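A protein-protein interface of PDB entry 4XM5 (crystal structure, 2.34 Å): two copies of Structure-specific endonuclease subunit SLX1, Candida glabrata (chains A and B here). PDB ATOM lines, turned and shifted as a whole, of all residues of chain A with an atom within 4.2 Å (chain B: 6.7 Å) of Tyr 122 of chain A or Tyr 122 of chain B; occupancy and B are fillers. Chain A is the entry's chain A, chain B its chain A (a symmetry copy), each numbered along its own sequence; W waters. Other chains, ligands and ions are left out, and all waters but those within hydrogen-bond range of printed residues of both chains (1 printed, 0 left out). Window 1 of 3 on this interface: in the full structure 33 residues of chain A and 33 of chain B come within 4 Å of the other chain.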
ATOM      1  N   GLU A 121     -12.140  18.977 -15.348  1.00  0.00           N
ATOM      2  CA  GLU A 121     -11.576  19.739 -14.239  1.00  0.00           C
ATOM      3  C   GLU A 121     -12.467  20.875 -13.795  1.00  0.00           C
ATOM      4  O   GLU A 121     -13.368  21.271 -14.518  1.00  0.00           O
ATOM      5  CB  GLU A 121     -10.221  20.308 -14.619  1.00  0.00           C
ATOM      6  CG  GLU A 121      -9.170  19.277 -14.850  1.00  0.00           C
ATOM      7  CD  GLU A 121      -8.652  18.721 -13.565  1.00  0.00           C
ATOM      8  OE1 GLU A 121      -7.738  17.879 -13.634  1.00  0.00           O
ATOM      9  OE2 GLU A 121      -9.150  19.141 -12.497  1.00  0.00           O
ATOM     10  N   TYR A 122     -12.195  21.415 -12.609  1.00  0.00           N
ATOM     11  CA  TYR A 122     -13.011  22.500 -12.051  1.00  0.00           C
ATOM     12  C   TYR A 122     -13.218  23.673 -13.025  1.00  0.00           C
ATOM     13  O   TYR A 122     -14.216  24.396 -12.928  1.00  0.00           O
ATOM     14  CB  TYR A 122     -12.399  23.009 -10.754  1.00  0.00           C
ATOM     15  CG  TYR A 122     -11.170  23.896 -10.864  1.00  0.00           C
ATOM     16  CD1 TYR A 122     -11.262  25.213 -11.315  1.00  0.00           C
ATOM     17  CD2 TYR A 122      -9.930  23.438 -10.440  1.00  0.00           C
ATOM     18  CE1 TYR A 122     -10.154  26.026 -11.387  1.00  0.00           C
ATOM     19  CE2 TYR A 122      -8.814  24.246 -10.484  1.00  0.00           C
ATOM     20  CZ  TYR A 122      -8.927  25.544 -10.961  1.00  0.00           C
ATOM     21  OH  TYR A 122      -7.820  26.364 -11.018  1.00  0.00           O
ATOM     22  N   PHE A 123     -12.280  23.856 -13.954  1.00  0.00           N
ATOM     23  CA  PHE A 123     -12.419  24.874 -14.982  1.00  0.00           C
ATOM     24  C   PHE A 123     -13.737  24.734 -15.722  1.00  0.00           C
ATOM     25  O   PHE A 123     -14.216  25.701 -16.315  1.00  0.00           O
ATOM     26  CB  PHE A 123     -11.262  24.807 -15.976  1.00  0.00           C
ATOM     27  CG  PHE A 123      -9.938  25.168 -15.382  1.00  0.00           C
ATOM     28  CD1 PHE A 123      -9.632  26.495 -15.093  1.00  0.00           C
ATOM     29  CD2 PHE A 123      -8.993  24.191 -15.113  1.00  0.00           C
ATOM     30  CE1 PHE A 123      -8.387  26.844 -14.530  1.00  0.00           C
ATOM     31  CE2 PHE A 123      -7.778  24.518 -14.570  1.00  0.00           C
ATOM     32  CZ  PHE A 123      -7.462  25.857 -14.272  1.00  0.00           C
ATOM     33  N   ARG A 124     -14.332  23.540 -15.664  1.00  0.00           N
ATOM     34  CA  ARG A 124     -15.552  23.229 -16.402  1.00  0.00           C
ATOM     35  C   ARG A 124     -16.661  24.177 -16.025  1.00  0.00           C
ATOM     36  O   ARG A 124     -17.624  24.352 -16.770  1.00  0.00           O
ATOM     37  CB  ARG A 124     -16.009  21.779 -16.158  1.00  0.00           C
ATOM     38  CG  ARG A 124     -16.449  21.472 -14.734  1.00  0.00           C
ATOM     39  CD  ARG A 124     -17.396  20.273 -14.677  1.00  0.00           C
ATOM     40  NE  ARG A 124     -16.718  18.998 -14.437  1.00  0.00           N
ATOM     41  CZ  ARG A 124     -16.658  18.384 -13.254  1.00  0.00           C
ATOM     42  NH1 ARG A 124     -17.232  18.921 -12.187  1.00  0.00           N
ATOM     43  NH2 ARG A 124     -16.021  17.224 -13.140  1.00  0.00           N
ATOM     44  N   TYR A 125     -16.531  24.791 -14.864  1.00  0.00           N
ATOM     45  CA  TYR A 125     -17.624  25.578 -14.348  1.00  0.00           C
ATOM     46  C   TYR A 125     -17.492  27.047 -14.723  1.00  0.00           C
ATOM     47  O   TYR A 125     -18.414  27.825 -14.533  1.00  0.00           O
ATOM     48  CB  TYR A 125     -17.712  25.389 -12.842  1.00  0.00           C
ATOM     49  CG  TYR A 125     -18.192  23.995 -12.464  1.00  0.00           C
ATOM     50  CD1 TYR A 125     -19.350  23.468 -13.017  1.00  0.00           C
ATOM     51  CD2 TYR A 125     -17.475  23.205 -11.564  1.00  0.00           C
ATOM     52  CE1 TYR A 125     -19.798  22.203 -12.680  1.00  0.00           C
ATOM     53  CE2 TYR A 125     -17.911  21.940 -11.216  1.00  0.00           C
ATOM     54  CZ  TYR A 125     -19.080  21.438 -11.778  1.00  0.00           C
ATOM     55  OH  TYR A 125     -19.531  20.171 -11.437  1.00  0.00           O
ATOM     56  N   MET A 126     -16.363  27.424 -15.297  1.00  0.00           N
ATOM     57  CA  MET A 126     -16.133  28.829 -15.615  1.00  0.00           C
ATOM     58  C   MET A 126     -16.723  29.382 -16.952  1.00  0.00           C
ATOM     59  O   MET A 126     -16.413  30.511 -17.323  1.00  0.00           O
ATOM     60  CB  MET A 126     -14.620  29.092 -15.596  1.00  0.00           C
ATOM     61  CG  MET A 126     -13.950  28.967 -14.209  1.00  0.00           C
ATOM     62  SD  MET A 126     -12.182  29.390 -14.367  1.00  0.00           S
ATOM     63  CE  MET A 126     -11.730  29.193 -12.632  1.00  0.00           C
ATOM     64  N   ILE A 272     -23.265  24.308  -6.857  1.00  0.00           N
ATOM     65  CA  ILE A 272     -22.907  25.670  -6.476  1.00  0.00           C
ATOM     66  C   ILE A 272     -22.775  26.651  -7.642  1.00  0.00           C
ATOM     67  O   ILE A 272     -22.684  27.852  -7.420  1.00  0.00           O
ATOM     68  CB  ILE A 272     -21.593  25.694  -5.675  1.00  0.00           C
ATOM     69  CG1 ILE A 272     -20.431  25.174  -6.520  1.00  0.00           C
ATOM     70  CG2 ILE A 272     -21.734  24.885  -4.414  1.00  0.00           C
ATOM     71  CD1 ILE A 272     -19.105  25.232  -5.818  1.00  0.00           C
ATOM     72  N   ILE B  73     -13.817  37.931  -7.440  1.00  0.00           N
ATOM     73  CA  ILE B  73     -14.817  37.129  -8.131  1.00  0.00           C
ATOM     74  C   ILE B  73     -15.020  35.792  -7.430  1.00  0.00           C
ATOM     75  O   ILE B  73     -16.155  35.372  -7.190  1.00  0.00           O
ATOM     76  CB  ILE B  73     -14.438  36.880  -9.613  1.00  0.00           C
ATOM     77  CG1 ILE B  73     -14.099  38.197 -10.298  1.00  0.00           C
ATOM     78  CG2 ILE B  73     -15.570  36.177 -10.357  1.00  0.00           C
ATOM     79  CD1 ILE B  73     -15.157  39.283 -10.121  1.00  0.00           C
ATOM     80  N   ALA B  74     -13.922  35.126  -7.096  1.00  0.00           N
ATOM     81  CA  ALA B  74     -14.025  33.849  -6.439  1.00  0.00           C
ATOM     82  C   ALA B  74     -14.656  33.993  -5.027  1.00  0.00           C
ATOM     83  O   ALA B  74     -15.427  33.129  -4.602  1.00  0.00           O
ATOM     84  CB  ALA B  74     -12.687  33.208  -6.384  1.00  0.00           C
ATOM     85  N   GLN B  77     -18.455  34.257  -5.520  1.00  0.00           N
ATOM     86  CA  GLN B  77     -19.111  32.993  -5.774  1.00  0.00           C
ATOM     87  C   GLN B  77     -19.182  32.049  -4.560  1.00  0.00           C
ATOM     88  O   GLN B  77     -20.132  31.276  -4.433  1.00  0.00           O
ATOM     89  CB  GLN B  77     -18.424  32.322  -6.940  1.00  0.00           C
ATOM     90  CG  GLN B  77     -18.571  33.183  -8.194  1.00  0.00           C
ATOM     91  CD  GLN B  77     -18.206  32.446  -9.427  1.00  0.00           C
ATOM     92  OE1 GLN B  77     -17.056  32.451  -9.830  1.00  0.00           O
ATOM     93  NE2 GLN B  77     -19.181  31.783 -10.034  1.00  0.00           N
ATOM     94  N   PHE B  78     -18.179  32.115  -3.682  1.00  0.00           N
ATOM     95  CA  PHE B  78     -18.211  31.404  -2.411  1.00  0.00           C
ATOM     96  C   PHE B  78     -19.415  31.941  -1.636  1.00  0.00           C
ATOM     97  O   PHE B  78     -20.246  31.180  -1.152  1.00  0.00           O
ATOM     98  CB  PHE B  78     -16.900  31.606  -1.636  1.00  0.00           C
ATOM     99  CG  PHE B  78     -16.723  30.680  -0.459  1.00  0.00           C
ATOM    100  CD1 PHE B  78     -17.183  31.036   0.800  1.00  0.00           C
ATOM    101  CD2 PHE B  78     -16.074  29.456  -0.615  1.00  0.00           C
ATOM    102  CE1 PHE B  78     -16.991  30.187   1.891  1.00  0.00           C
ATOM    103  CE2 PHE B  78     -15.881  28.602   0.446  1.00  0.00           C
ATOM    104  CZ  PHE B  78     -16.342  28.959   1.708  1.00  0.00           C
ATOM    105  N   SER B 116     -19.074  21.879   3.234  1.00  0.00           N
ATOM    106  CA  SER B 116     -19.430  21.495   1.885  1.00  0.00           C
ATOM    107  C   SER B 116     -18.508  22.177   0.866  1.00  0.00           C
ATOM    108  O   SER B 116     -17.856  21.509   0.066  1.00  0.00           O
ATOM    109  CB  SER B 116     -20.888  21.856   1.627  1.00  0.00           C
ATOM    110  OG  SER B 116     -21.428  21.042   0.610  1.00  0.00           O
ATOM    111  N   LEU B 117     -18.426  23.505   0.940  1.00  0.00           N
ATOM    112  CA  LEU B 117     -17.643  24.304  -0.006  1.00  0.00           C
ATOM    113  C   LEU B 117     -16.139  24.042   0.080  1.00  0.00           C
ATOM    114  O   LEU B 117     -15.459  23.907  -0.956  1.00  0.00           O
ATOM    115  CB  LEU B 117     -17.924  25.796   0.203  1.00  0.00           C
ATOM    116  CG  LEU B 117     -19.383  26.213  -0.057  1.00  0.00           C
ATOM    117  CD1 LEU B 117     -19.750  27.616   0.510  1.00  0.00           C
ATOM    118  CD2 LEU B 117     -19.709  26.101  -1.563  1.00  0.00           C
ATOM    119  N   LEU B 118     -15.615  23.954   1.299  1.00  0.00           N
ATOM    120  CA  LEU B 118     -14.173  23.796   1.486  1.00  0.00           C
ATOM    121  C   LEU B 118     -13.686  22.371   1.226  1.00  0.00           C
ATOM    122  O   LEU B 118     -12.616  22.166   0.660  1.00  0.00           O
ATOM    123  CB  LEU B 118     -13.757  24.206   2.899  1.00  0.00           C
ATOM    124  CG  LEU B 118     -13.748  25.685   3.279  1.00  0.00           C
ATOM    125  CD1 LEU B 118     -13.349  25.817   4.757  1.00  0.00           C
ATOM    126  CD2 LEU B 118     -12.828  26.536   2.372  1.00  0.00           C
ATOM    127  N   ASN B 120     -15.611  19.528  -0.015  1.00  0.00           N
ATOM    128  CA  ASN B 120     -16.193  18.741  -1.105  1.00  0.00           C
ATOM    129  C   ASN B 120     -16.259  19.463  -2.454  1.00  0.00           C
ATOM    130  O   ASN B 120     -16.656  18.865  -3.462  1.00  0.00           O
ATOM    131  CB  ASN B 120     -17.608  18.273  -0.723  1.00  0.00           C
ATOM    132  CG  ASN B 120     -17.628  17.408   0.538  1.00  0.00           C
ATOM    133  OD1 ASN B 120     -16.591  16.929   1.001  1.00  0.00           O
ATOM    134  ND2 ASN B 120     -18.822  17.198   1.088  1.00  0.00           N
ATOM    135  N   GLU B 121     -15.883  20.735  -2.473  1.00  0.00           N
ATOM    136  CA  GLU B 121     -16.032  21.547  -3.676  1.00  0.00           C
ATOM    137  C   GLU B 121     -14.710  22.040  -4.217  1.00  0.00           C
ATOM    138  O   GLU B 121     -13.711  22.020  -3.517  1.00  0.00           O
ATOM    139  CB  GLU B 121     -16.920  22.748  -3.402  1.00  0.00           C
ATOM    140  CG  GLU B 121     -18.334  22.400  -3.089  1.00  0.00           C
ATOM    141  CD  GLU B 121     -19.096  22.032  -4.319  1.00  0.00           C
ATOM    142  OE1 GLU B 121     -20.304  21.763  -4.183  1.00  0.00           O
ATOM    143  OE2 GLU B 121     -18.489  22.031  -5.412  1.00  0.00           O
ATOM    144  N   TYR B 122     -14.717  22.508  -5.464  1.00  0.00           N
ATOM    145  CA  TYR B 122     -13.489  22.981  -6.115  1.00  0.00           C
ATOM    146  C   TYR B 122     -12.703  24.000  -5.272  1.00  0.00           C
ATOM    147  O   TYR B 122     -11.482  24.123  -5.420  1.00  0.00           O
ATOM    148  CB  TYR B 122     -13.810  23.577  -7.478  1.00  0.00           C
ATOM    149  CG  TYR B 122     -14.439  24.960  -7.504  1.00  0.00           C
ATOM    150  CD1 TYR B 122     -13.697  26.102  -7.199  1.00  0.00           C
ATOM    151  CD2 TYR B 122     -15.756  25.128  -7.911  1.00  0.00           C
ATOM    152  CE1 TYR B 122     -14.259  27.357  -7.252  1.00  0.00           C
ATOM    153  CE2 TYR B 122     -16.328  26.379  -7.990  1.00  0.00           C
ATOM    154  CZ  TYR B 122     -15.577  27.497  -7.657  1.00  0.00           C
ATOM    155  OH  TYR B 122     -16.135  28.757  -7.724  1.00  0.00           O
ATOM    156  N   PHE B 123     -13.402  24.724  -4.397  1.00  0.00           N
ATOM    157  CA  PHE B 123     -12.750  25.649  -3.485  1.00  0.00           C
ATOM    158  C   PHE B 123     -11.650  24.962  -2.696  1.00  0.00           C
ATOM    159  O   PHE B 123     -10.740  25.627  -2.200  1.00  0.00           O
ATOM    160  CB  PHE B 123     -13.760  26.271  -2.525  1.00  0.00           C
ATOM    161  CG  PHE B 123     -14.752  27.168  -3.194  1.00  0.00           C
ATOM    162  CD1 PHE B 123     -14.374  28.432  -3.638  1.00  0.00           C
ATOM    163  CD2 PHE B 123     -16.063  26.759  -3.380  1.00  0.00           C
ATOM    164  CE1 PHE B 123     -15.302  29.283  -4.272  1.00  0.00           C
ATOM    165  CE2 PHE B 123     -16.975  27.579  -3.992  1.00  0.00           C
ATOM    166  CZ  PHE B 123     -16.600  28.857  -4.446  1.00  0.00           C
ATOM    167  N   ARG B 124     -11.722  23.632  -2.603  1.00  0.00           N
ATOM    168  CA  ARG B 124     -10.791  22.845  -1.799  1.00  0.00           C
ATOM    169  C   ARG B 124      -9.371  23.076  -2.247  1.00  0.00           C
ATOM    170  O   ARG B 124      -8.426  22.837  -1.498  1.00  0.00           O
ATOM    171  CB  ARG B 124     -11.114  21.341  -1.866  1.00  0.00           C
ATOM    172  CG  ARG B 124     -10.925  20.701  -3.234  1.00  0.00           C
ATOM    173  CD  ARG B 124     -10.692  19.193  -3.129  1.00  0.00           C
ATOM    174  NE  ARG B 124     -11.916  18.400  -3.246  1.00  0.00           N
ATOM    175  CZ  ARG B 124     -12.306  17.768  -4.354  1.00  0.00           C
ATOM    176  NH1 ARG B 124     -11.574  17.829  -5.457  1.00  0.00           N
ATOM    177  NH2 ARG B 124     -13.434  17.066  -4.357  1.00  0.00           N
ATOM    178  N   TYR B 125      -9.216  23.540  -3.472  1.00  0.00           N
ATOM    179  CA  TYR B 125      -7.893  23.625  -4.041  1.00  0.00           C
ATOM    180  C   TYR B 125      -7.274  25.000  -3.836  1.00  0.00           C
ATOM    181  O   TYR B 125      -6.095  25.197  -4.083  1.00  0.00           O
ATOM    182  CB  TYR B 125      -7.955  23.251  -5.513  1.00  0.00           C
ATOM    183  CG  TYR B 125      -8.234  21.769  -5.719  1.00  0.00           C
ATOM    184  CD1 TYR B 125      -7.469  20.806  -5.077  1.00  0.00           C
ATOM    185  CD2 TYR B 125      -9.273  21.339  -6.546  1.00  0.00           C
ATOM    186  CE1 TYR B 125      -7.711  19.455  -5.258  1.00  0.00           C
ATOM    187  CE2 TYR B 125      -9.526  19.993  -6.738  1.00  0.00           C
ATOM    188  CZ  TYR B 125      -8.740  19.048  -6.089  1.00  0.00           C
ATOM    189  OH  TYR B 125      -8.980  17.694  -6.274  1.00  0.00           O
ATOM    190  N   MET B 126      -8.054  25.945  -3.340  1.00  0.00           N
ATOM    191  CA  MET B 126      -7.554  27.307  -3.188  1.00  0.00           C
ATOM    192  C   MET B 126      -6.729  27.643  -1.905  1.00  0.00           C
ATOM    193  O   MET B 126      -6.432  28.812  -1.670  1.00  0.00           O
ATOM    194  CB  MET B 126      -8.741  28.276  -3.281  1.00  0.00           C
ATOM    195  CG  MET B 126      -9.426  28.343  -4.665  1.00  0.00           C
ATOM    196  SD  MET B 126     -10.752  29.596  -4.606  1.00  0.00           S
ATOM    197  CE  MET B 126     -11.293  29.455  -6.321  1.00  0.00           C
ATOM    198  N   ILE B 272      -3.831  18.919 -11.174  1.00  0.00           N
ATOM    199  CA  ILE B 272      -3.483  20.228 -11.715  1.00  0.00           C
ATOM    200  C   ILE B 272      -3.081  21.270 -10.670  1.00  0.00           C
ATOM    201  O   ILE B 272      -2.576  22.327 -11.027  1.00  0.00           O
ATOM    202  CB  ILE B 272      -4.638  20.806 -12.552  1.00  0.00           C
ATOM    203  CG1 ILE B 272      -5.880  21.023 -11.689  1.00  0.00           C
ATOM    204  CG2 ILE B 272      -4.951  19.898 -13.711  1.00  0.00           C
ATOM    205  CD1 ILE B 272      -7.026  21.647 -12.432  1.00  0.00           C
ATOM    206  N   ILE B 273      -3.310  20.986  -9.394  1.00  0.00           N
ATOM    207  CA  ILE B 273      -2.782  21.846  -8.339  1.00  0.00           C
ATOM    208  C   ILE B 273      -2.080  21.007  -7.276  1.00  0.00           C
ATOM    209  O   ILE B 273      -2.643  20.027  -6.793  1.00  0.00           O
ATOM    210  CB  ILE B 273      -3.892  22.701  -7.695  1.00  0.00           C
ATOM    211  CG1 ILE B 273      -4.347  23.778  -8.679  1.00  0.00           C
ATOM    212  CG2 ILE B 273      -3.400  23.372  -6.460  1.00  0.00           C
ATOM    213  CD1 ILE B 273      -5.053  24.943  -8.044  1.00  0.00           C
HETATM  214  O   HOH W   1     -21.380  30.317  -6.881  1.00  0.00           O
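O of Ser 116 of chain B sits at hydrogen-bond distance from N of Glu 121 of chain B, at 3.3 Å.
Among the printed residues, merely in contact across the chains: Glu 121 of chain A with Ile 272 of chain B (3.3 Å), Tyr 122 of chain A with Tyr 122 of chain B (3.6 Å), Tyr 122 of chain A with Ile 272 of chain B (3.7 Å), Phe 123 of chain A with Ile 272 of chain B (3.7 Å), Ile 272 of chain A with Leu 117 of chain B (3.7 Å), Ile 272 of chain A with Glu 121 of chain B (3.3 Å), Ile 272 of chain A with Tyr 122 of chain B (3.7 Å) and Ile 272 of chain A with Phe 123 of chain B (3.7 Å).
Of the printed residues of chain B, Glu 121 of chain A touches Ile 272 (3.3 Å). Tyr 122 of chain A touches just these residues of chain B: Tyr 122 and Ile 272. Printed residues of chain A within 4 Å of Glu 121 of chain B: Ile 272 (3.3 Å).
Of the 16 printed residues of chain B, 5 touch a printed residue of chain A. Printed residues of chain B that touch a printed residue of chain A: Leu 117, Glu 121, Tyr 122, Phe 123 and Ile 272. Hydrophobic or aromatic side chains of chain B that line the printed part of chain A: Leu 117, Tyr 122, Phe 123 and Ile 272.
Glu 121 of chain A touches Ile 272 of chain B, and with the chains exchanged Ile 272 of chain A touches Glu 121 of chain B. Tyr 122 of chain B touches its own counterpart, Tyr 122 of chain A. Tyr 122 of chain A touches Ile 272 of chain B, and with the chains exchanged Ile 272 of chain A touches Tyr 122 of chain B. Phe 123 of chain A touches Ile 272 of chain B, and with the chains exchanged Ile 272 of chain A touches Phe 123 of chain B. Positions printed for both chains: 121, 122, 123, 124, 125, 126 and 272.
Water W1 bridges O of Ile 272 of chain A (2.8 Å) and O of Gln 77 of chain B (2.9 Å).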
